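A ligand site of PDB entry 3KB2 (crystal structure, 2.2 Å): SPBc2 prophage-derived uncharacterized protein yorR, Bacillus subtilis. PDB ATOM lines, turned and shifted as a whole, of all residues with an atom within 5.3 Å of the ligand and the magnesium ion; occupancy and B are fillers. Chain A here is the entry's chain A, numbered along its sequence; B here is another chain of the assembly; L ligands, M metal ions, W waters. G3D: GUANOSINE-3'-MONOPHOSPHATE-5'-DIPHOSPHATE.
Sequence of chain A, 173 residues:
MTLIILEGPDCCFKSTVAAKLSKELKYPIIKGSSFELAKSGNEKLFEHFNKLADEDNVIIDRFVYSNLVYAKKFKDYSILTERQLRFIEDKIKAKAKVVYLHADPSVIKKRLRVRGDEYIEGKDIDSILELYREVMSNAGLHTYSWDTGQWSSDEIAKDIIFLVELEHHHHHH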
ATOM      1  N   PRO A   9      35.167 -12.646 -25.391  1.00  0.00           N
ATOM      2  CA  PRO A   9      35.080 -13.871 -24.600  1.00  0.00           C
ATOM      3  C   PRO A   9      33.734 -13.979 -23.880  1.00  0.00           C
ATOM      4  O   PRO A   9      32.969 -13.026 -23.837  1.00  0.00           O
ATOM      5  CB  PRO A   9      36.238 -13.721 -23.620  1.00  0.00           C
ATOM      6  CG  PRO A   9      36.285 -12.232 -23.397  1.00  0.00           C
ATOM      7  CD  PRO A   9      36.184 -11.742 -24.831  1.00  0.00           C
ATOM      8  N   ASP A  10      33.480 -15.151 -23.300  1.00  0.00           N
ATOM      9  CA  ASP A  10      32.246 -15.416 -22.571  1.00  0.00           C
ATOM     10  C   ASP A  10      32.011 -14.511 -21.370  1.00  0.00           C
ATOM     11  O   ASP A  10      32.956 -13.960 -20.786  1.00  0.00           O
ATOM     12  CB  ASP A  10      32.238 -16.849 -22.063  1.00  0.00           C
ATOM     13  CG  ASP A  10      32.052 -17.863 -23.161  1.00  0.00           C
ATOM     14  OD1 ASP A  10      31.935 -19.062 -22.834  1.00  0.00           O
ATOM     15  OD2 ASP A  10      32.008 -17.457 -24.351  1.00  0.00           O
ATOM     16  N   CYS A  11      30.749 -14.375 -21.006  1.00  0.00           N
ATOM     17  CA  CYS A  11      30.365 -13.572 -19.855  1.00  0.00           C
ATOM     18  C   CYS A  11      30.784 -12.117 -19.935  1.00  0.00           C
ATOM     19  O   CYS A  11      31.201 -11.522 -18.938  1.00  0.00           O
ATOM     20  CB  CYS A  11      30.936 -14.219 -18.589  1.00  0.00           C
ATOM     21  SG  CYS A  11      30.273 -15.863 -18.300  1.00  0.00           S
ATOM     22  N   CYS A  12      30.676 -11.530 -21.125  1.00  0.00           N
ATOM     23  CA  CYS A  12      31.033 -10.139 -21.295  1.00  0.00           C
ATOM     24  C   CYS A  12      29.846  -9.331 -21.788  1.00  0.00           C
ATOM     25  O   CYS A  12      30.011  -8.345 -22.507  1.00  0.00           O
ATOM     26  CB  CYS A  12      32.235  -9.996 -22.248  1.00  0.00           C
ATOM     27  SG  CYS A  12      33.804 -10.563 -21.517  1.00  0.00           S
ATOM     28  N   PHE A  13      28.651  -9.755 -21.389  1.00  0.00           N
ATOM     29  CA  PHE A  13      27.421  -9.081 -21.722  1.00  0.00           C
ATOM     30  C   PHE A  13      27.017  -9.082 -23.198  1.00  0.00           C
ATOM     31  O   PHE A  13      26.080  -8.382 -23.575  1.00  0.00           O
ATOM     32  CB  PHE A  13      27.480  -7.618 -21.218  1.00  0.00           C
ATOM     33  CG  PHE A  13      27.921  -7.460 -19.775  1.00  0.00           C
ATOM     34  CD1 PHE A  13      27.841  -8.517 -18.869  1.00  0.00           C
ATOM     35  CD2 PHE A  13      28.359  -6.218 -19.289  1.00  0.00           C
ATOM     36  CE1 PHE A  13      28.175  -8.348 -17.519  1.00  0.00           C
ATOM     37  CE2 PHE A  13      28.703  -6.050 -17.941  1.00  0.00           C
ATOM     38  CZ  PHE A  13      28.614  -7.108 -17.065  1.00  0.00           C
ATOM     39  N   LYS A  14      27.703  -9.865 -24.018  1.00  0.00           N
ATOM     40  CA  LYS A  14      27.383  -9.882 -25.448  1.00  0.00           C
ATOM     41  C   LYS A  14      25.906 -10.115 -25.771  1.00  0.00           C
ATOM     42  O   LYS A  14      25.293  -9.303 -26.453  1.00  0.00           O
ATOM     43  CB  LYS A  14      28.254 -10.912 -26.183  1.00  0.00           C
ATOM     44  CG  LYS A  14      29.747 -10.591 -26.062  1.00  0.00           C
ATOM     45  CD  LYS A  14      30.585 -11.335 -27.098  1.00  0.00           C
ATOM     46  CE  LYS A  14      30.299 -12.827 -27.090  1.00  0.00           C
ATOM     47  NZ  LYS A  14      30.429 -13.362 -25.726  1.00  0.00           N
ATOM     48  N   SER A  15      25.351 -11.204 -25.259  1.00  0.00           N
ATOM     49  CA  SER A  15      23.952 -11.534 -25.527  1.00  0.00           C
ATOM     50  C   SER A  15      22.950 -10.566 -24.907  1.00  0.00           C
ATOM     51  O   SER A  15      21.865 -10.331 -25.460  1.00  0.00           O
ATOM     52  CB  SER A  15      23.680 -12.953 -25.075  1.00  0.00           C
ATOM     53  OG  SER A  15      24.389 -13.841 -25.920  1.00  0.00           O
ATOM     54  N   THR A  16      23.311 -10.021 -23.753  1.00  0.00           N
ATOM     55  CA  THR A  16      22.479  -9.062 -23.038  1.00  0.00           C
ATOM     56  C   THR A  16      22.471  -7.785 -23.895  1.00  0.00           C
ATOM     57  O   THR A  16      21.409  -7.253 -24.207  1.00  0.00           O
ATOM     58  CB  THR A  16      23.077  -8.755 -21.653  1.00  0.00           C
ATOM     59  OG1 THR A  16      23.185  -9.969 -20.915  1.00  0.00           O
ATOM     60  CG2 THR A  16      22.192  -7.783 -20.871  1.00  0.00           C
ATOM     61  N   VAL A  17      23.649  -7.307 -24.262  1.00  0.00           N
ATOM     62  CA  VAL A  17      23.737  -6.101 -25.080  1.00  0.00           C
ATOM     63  C   VAL A  17      22.915  -6.298 -26.336  1.00  0.00           C
ATOM     64  O   VAL A  17      22.119  -5.440 -26.712  1.00  0.00           O
ATOM     65  CB  VAL A  17      25.188  -5.767 -25.459  1.00  0.00           C
ATOM     66  CG1 VAL A  17      25.212  -4.696 -26.540  1.00  0.00           C
ATOM     67  CG2 VAL A  17      25.927  -5.274 -24.237  1.00  0.00           C
ATOM     68  N   LYS A  31      23.079 -15.564 -34.031  1.00  0.00           N
ATOM     69  CA  LYS A  31      24.345 -16.077 -33.513  1.00  0.00           C
ATOM     70  C   LYS A  31      25.207 -16.409 -34.734  1.00  0.00           C
ATOM     71  O   LYS A  31      24.767 -17.151 -35.606  1.00  0.00           O
ATOM     72  CB  LYS A  31      24.105 -17.345 -32.693  1.00  0.00           C
ATOM     73  CG  LYS A  31      23.189 -17.151 -31.506  1.00  0.00           C
ATOM     74  CD  LYS A  31      23.876 -16.359 -30.396  1.00  0.00           C
ATOM     75  CE  LYS A  31      24.327 -17.268 -29.243  1.00  0.00           C
ATOM     76  NZ  LYS A  31      25.358 -18.280 -29.625  1.00  0.00           N
ATOM     77  N   ASP A  61      25.649 -11.923 -32.819  1.00  0.00           N
ATOM     78  CA  ASP A  61      26.240 -12.302 -31.543  1.00  0.00           C
ATOM     79  C   ASP A  61      27.335 -13.326 -31.840  1.00  0.00           C
ATOM     80  O   ASP A  61      27.046 -14.505 -31.998  1.00  0.00           O
ATOM     81  CB  ASP A  61      25.144 -12.898 -30.640  1.00  0.00           C
ATOM     82  CG  ASP A  61      25.589 -13.121 -29.196  1.00  0.00           C
ATOM     83  OD1 ASP A  61      24.712 -13.407 -28.371  1.00  0.00           O
ATOM     84  OD2 ASP A  61      26.798 -13.000 -28.895  1.00  0.00           O
ATOM     85  N   ARG A 115      28.438 -18.245 -12.452  1.00  0.00           N
ATOM     86  CA  ARG A 115      27.616 -18.886 -13.463  1.00  0.00           C
ATOM     87  C   ARG A 115      27.466 -20.364 -13.116  1.00  0.00           C
ATOM     88  O   ARG A 115      26.467 -21.004 -13.442  1.00  0.00           O
ATOM     89  CB  ARG A 115      28.265 -18.742 -14.841  1.00  0.00           C
ATOM     90  CG  ARG A 115      27.514 -19.477 -15.940  1.00  0.00           C
ATOM     91  CD  ARG A 115      28.478 -20.104 -16.945  1.00  0.00           C
ATOM     92  NE  ARG A 115      28.634 -19.305 -18.159  1.00  0.00           N
ATOM     93  CZ  ARG A 115      29.375 -19.686 -19.193  1.00  0.00           C
ATOM     94  NH1 ARG A 115      30.022 -20.840 -19.174  1.00  0.00           N
ATOM     95  NH2 ARG A 115      29.454 -18.901 -20.267  1.00  0.00           N
ATOM     96  N   TRP A 151      31.769  -1.102 -17.310  1.00  0.00           N
ATOM     97  CA  TRP A 151      30.676  -0.614 -18.138  1.00  0.00           C
ATOM     98  C   TRP A 151      29.535  -1.612 -18.129  1.00  0.00           C
ATOM     99  O   TRP A 151      29.741  -2.788 -18.419  1.00  0.00           O
ATOM    100  CB  TRP A 151      31.172  -0.422 -19.563  1.00  0.00           C
ATOM    101  CG  TRP A 151      31.388   0.969 -19.945  1.00  0.00           C
ATOM    102  CD1 TRP A 151      30.454   1.836 -20.447  1.00  0.00           C
ATOM    103  CD2 TRP A 151      32.606   1.709 -19.842  1.00  0.00           C
ATOM    104  NE1 TRP A 151      31.017   3.057 -20.677  1.00  0.00           N
ATOM    105  CE2 TRP A 151      32.342   3.019 -20.311  1.00  0.00           C
ATOM    106  CE3 TRP A 151      33.890   1.388 -19.409  1.00  0.00           C
ATOM    107  CZ2 TRP A 151      33.317   4.006 -20.354  1.00  0.00           C
ATOM    108  CZ3 TRP A 151      34.877   2.378 -19.445  1.00  0.00           C
ATOM    109  CH2 TRP A 151      34.579   3.675 -19.920  1.00  0.00           C
ATOM    110  N   SER A 152      28.316  -1.160 -17.801  1.00  0.00           N
ATOM    111  CA  SER A 152      27.151  -2.053 -17.766  1.00  0.00           C
ATOM    112  C   SER A 152      26.533  -2.254 -19.150  1.00  0.00           C
ATOM    113  O   SER A 152      26.748  -1.437 -20.046  1.00  0.00           O
ATOM    114  CB  SER A 152      26.080  -1.490 -16.827  1.00  0.00           C
ATOM    115  OG  SER A 152      25.451  -0.369 -17.415  1.00  0.00           O
ATOM    116  N   SER A 153      25.757  -3.314 -19.342  1.00  0.00           N
ATOM    117  CA  SER A 153      25.147  -3.561 -20.646  1.00  0.00           C
ATOM    118  C   SER A 153      24.233  -2.420 -21.064  1.00  0.00           C
ATOM    119  O   SER A 153      24.036  -2.184 -22.257  1.00  0.00           O
ATOM    120  CB  SER A 153      24.395  -4.905 -20.679  1.00  0.00           C
ATOM    121  OG  SER A 153      23.442  -5.005 -19.631  1.00  0.00           O
ATOM    122  N   ASP A 154      23.651  -1.716 -20.105  1.00  0.00           N
ATOM    123  CA  ASP A 154      22.803  -0.575 -20.433  1.00  0.00           C
ATOM    124  C   ASP A 154      23.650   0.534 -21.031  1.00  0.00           C
ATOM    125  O   ASP A 154      23.357   1.047 -22.104  1.00  0.00           O
ATOM    126  CB  ASP A 154      22.094  -0.034 -19.189  1.00  0.00           C
ATOM    127  CG  ASP A 154      20.751  -0.663 -18.950  1.00  0.00           C
ATOM    128  OD1 ASP A 154      20.024  -0.201 -18.048  1.00  0.00           O
ATOM    129  OD2 ASP A 154      20.403  -1.618 -19.676  1.00  0.00           O
ATOM    130  N   VAL B 114      22.510 -23.625 -17.789  1.00  0.00           N
ATOM    131  CA  VAL B 114      23.130 -22.374 -17.361  1.00  0.00           C
ATOM    132  C   VAL B 114      23.110 -21.398 -18.528  1.00  0.00           C
ATOM    133  O   VAL B 114      23.110 -20.184 -18.338  1.00  0.00           O
ATOM    134  CB  VAL B 114      24.584 -22.577 -16.922  1.00  0.00           C
ATOM    135  CG1 VAL B 114      24.647 -23.512 -15.728  1.00  0.00           C
ATOM    136  CG2 VAL B 114      25.409 -23.129 -18.076  1.00  0.00           C
ATOM    137  N   ARG B 115      23.096 -21.955 -19.741  1.00  0.00           N
ATOM    138  CA  ARG B 115      23.083 -21.169 -20.964  1.00  0.00           C
ATOM    139  C   ARG B 115      23.237 -22.101 -22.185  1.00  0.00           C
ATOM    140  O   ARG B 115      24.224 -22.837 -22.298  1.00  0.00           O
ATOM    141  CB  ARG B 115      24.223 -20.151 -20.947  1.00  0.00           C
ATOM    142  CG  ARG B 115      23.860 -18.764 -21.501  1.00  0.00           C
ATOM    143  CD  ARG B 115      23.384 -18.821 -22.957  1.00  0.00           C
ATOM    144  NE  ARG B 115      22.933 -17.509 -23.424  1.00  0.00           N
ATOM    145  CZ  ARG B 115      21.890 -16.845 -22.916  1.00  0.00           C
ATOM    146  NH1 ARG B 115      21.182 -17.367 -21.916  1.00  0.00           N
ATOM    147  NH2 ARG B 115      21.555 -15.660 -23.407  1.00  0.00           N
ATOM    148  N   ASP B 117      24.335 -21.780 -24.881  1.00  0.00           N
ATOM    149  CA  ASP B 117      25.580 -21.593 -25.619  1.00  0.00           C
ATOM    150  C   ASP B 117      26.683 -22.537 -25.153  1.00  0.00           C
ATOM    151  O   ASP B 117      27.471 -23.025 -25.975  1.00  0.00           O
ATOM    152  CB  ASP B 117      26.068 -20.138 -25.488  1.00  0.00           C
ATOM    153  CG  ASP B 117      26.762 -19.860 -24.155  1.00  0.00           C
ATOM    154  OD1 ASP B 117      26.193 -20.212 -23.093  1.00  0.00           O
ATOM    155  OD2 ASP B 117      27.889 -19.300 -24.171  1.00  0.00           O
HETATM  156  PB  G3D L   1      27.760 -13.475 -22.828  1.00  0.00           P
HETATM  157  O1B G3D L   1      28.481 -14.799 -22.629  1.00  0.00           O
HETATM  158  O2B G3D L   1      28.529 -12.357 -23.372  1.00  0.00           O
HETATM  159  O3B G3D L   1      26.447 -13.756 -23.792  1.00  0.00           O
HETATM  160  PA  G3D L   1      25.574 -12.489 -21.251  1.00  0.00           P
HETATM  161  O3A G3D L   1      27.062 -13.035 -21.508  1.00  0.00           O
HETATM  162  O1A G3D L   1      25.287 -11.288 -22.028  1.00  0.00           O
HETATM  163  O2A G3D L   1      24.639 -13.702 -21.396  1.00  0.00           O
HETATM  164  O5' G3D L   1      25.682 -11.983 -19.674  1.00  0.00           O
HETATM  165  C5' G3D L   1      26.415 -12.993 -18.859  1.00  0.00           C
HETATM  166  C4' G3D L   1      25.783 -12.563 -17.446  1.00  0.00           C
HETATM  167  O4' G3D L   1      26.138 -11.254 -16.980  1.00  0.00           O
HETATM  168  C3' G3D L   1      24.356 -12.629 -17.268  1.00  0.00           C
HETATM  169  O3' G3D L   1      23.991 -13.234 -16.047  1.00  0.00           O
HETATM  170  C2' G3D L   1      23.725 -11.227 -17.513  1.00  0.00           C
HETATM  171  O2' G3D L   1      22.621 -11.037 -16.818  1.00  0.00           O
HETATM  172  C1' G3D L   1      24.990 -10.477 -16.633  1.00  0.00           C
HETATM  173  N9  G3D L   1      24.940  -8.998 -16.952  1.00  0.00           N
HETATM  174  C8  G3D L   1      24.418  -8.493 -18.139  1.00  0.00           C
HETATM  175  N7  G3D L   1      24.642  -7.184 -17.886  1.00  0.00           N
HETATM  176  C5  G3D L   1      25.105  -6.874 -16.614  1.00  0.00           C
HETATM  177  C6  G3D L   1      25.354  -5.748 -16.128  1.00  0.00           C
HETATM  178  O6  G3D L   1      25.357  -4.519 -16.463  1.00  0.00           O
HETATM  179  N1  G3D L   1      25.965  -5.880 -14.756  1.00  0.00           N
HETATM  180  C2  G3D L   1      26.069  -7.091 -14.339  1.00  0.00           C
HETATM  181  N2  G3D L   1      26.744  -7.215 -13.002  1.00  0.00           N
HETATM  182  N3  G3D L   1      25.880  -8.282 -14.888  1.00  0.00           N
HETATM  183  C4  G3D L   1      25.311  -8.049 -16.065  1.00  0.00           C
HETATM  184  P1  G3D L   1      23.163 -14.288 -15.861  1.00  0.00           P
HETATM  185  O4P G3D L   1      21.822 -13.868 -15.627  1.00  0.00           O
HETATM  186  O5P G3D L   1      23.753 -14.902 -14.501  1.00  0.00           O
HETATM  187  O6P G3D L   1      23.332 -15.520 -16.760  1.00  0.00           O
HETATM  188 MG    MG M   1      26.031 -15.346 -25.290  1.00  0.00          MG
HETATM  189  O   HOH W   1      27.403 -14.576 -26.925  1.00  0.00           O
HETATM  190  O   HOH W   2      24.659 -15.329 -23.380  1.00  0.00           O
HETATM  191  O   HOH W   3      27.536 -16.158 -20.465  1.00  0.00           O
HETATM  192  O   HOH W   4      22.788  -2.868 -17.565  1.00  0.00           O
HETATM  193  O   HOH W   5      27.807 -16.521 -24.563  1.00  0.00           O
HETATM  194  O   HOH W   6      27.114 -11.323 -13.689  1.00  0.00           O
HETATM  195  O   HOH W   7      20.967 -16.363 -17.322  1.00  0.00           O
HETATM  196  O   HOH W   8      24.957 -17.252 -25.986  1.00  0.00           O
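O1A of the ligand sits at hydrogen-bond distance from N of Ser 15, at 3.2 Å. An oxygen (O2B) of the ligand lies within hydrogen-bond range of the backbone NH (N) of Lys 14 (2.7 Å). NZ of Lys 14 is in salt-bridge range of O2B of the ligand, at 3.2 Å. N of Thr 16 lies within hydrogen-bond range of O1A of the ligand (2.9 Å). An oxygen (O1A) of the ligand sits at hydrogen-bond distance from the side-chain hydroxyl (OG1) of Thr 16 (2.7 Å). N of Cys 11 lies within hydrogen-bond range of O1B of the ligand, at 2.8 Å. An oxygen (O2B) of the ligand sits at hydrogen-bond distance from the backbone NH (N) of Phe 13 (3.3 Å). An oxygen (O6) of the ligand lies within hydrogen-bond range of the backbone NH (N) of Ser 153 (3.1 Å). OG of Ser 153 is in hydrogen-bond range of N7 of the ligand, 3.0 Å away. N of Cys 12 sits at hydrogen-bond distance from O2B of the ligand.
The side-chain carboxylate (OD1) of Asp 61 lies close to the side-chain hydroxyl (OG) of Ser 15, at 2.5 Å. The side-chain amino group (NZ) of Lys 14 lies within hydrogen-bond range of the backbone carbonyl oxygen (O) of Pro 9. The side-chain sulfur (SG) of Cys 11 is in hydrogen-bond range of the guanidinium group (NH2) of Arg 115 of chain A, at 3.7 Å. SG of Cys 12 sits at hydrogen-bond distance from O of Asp 10 (3.6 Å). The side-chain sulfur (SG) of Cys 12 sits at hydrogen-bond distance from the backbone carbonyl oxygen (O) of Pro 9. The guanidinium group (NH2) of Arg 115 of chain A lies within salt-bridge range of the side-chain carboxylate (OD1) of Asp 10, at 3.6 Å.
Asp 10 touches the ligand. Ser 152 touches the ligand (CB to O6, 3.1 Å). Hydrophobic or aromatic side chains within 4 Å of the ligand: Phe 13. Within 4 Å of the ligand: Asp 10, Cys 11, Cys 12, Phe 13, Lys 14, Ser 15, Thr 16, Ser 152 and Ser 153. The nearest printed residue that does not touch the ligand is Arg 115 of chain B (4.2 Å).
Merely in contact with the magnesium ion: Asp 61 (3.9 Å). Two residues have an atom within 4 Å of the magnesium ion: Ser 15 and Asp 61.
The magnesium ion is bound by an oxygen (O3B) of the ligand (2.2 Å), water W5 (2.3 Å), water W1 (2.3 Å), water W8 (2.3 Å), the side-chain hydroxyl (OG) of Ser 15 (2.3 Å) and water W2 (2.4 Å).
Water W2 lies within hydrogen-bond range of O2A of the ligand (2.6 Å) and NE of Arg 115 of chain B (2.8 Å). Water W5 lies within hydrogen-bond range of O1B of the ligand (2.7 Å) and OD2 of Asp 117 of chain B (2.8 Å). Water W1 lies within hydrogen-bond range of OD2 of Asp 61 (2.6 Å) and NZ of Lys 14 (3.5 Å). Water W3 lies within hydrogen-bond range of an oxygen (O1B) of the ligand (2.7 Å), the guanidinium group of Arg 115 of chain A (3.4 Å) and the side-chain sulfur of Cys 11 (3.5 Å). Water W4 lies within hydrogen-bond range of N of Asp 154, OG of Ser 153 and O6 of the ligand.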
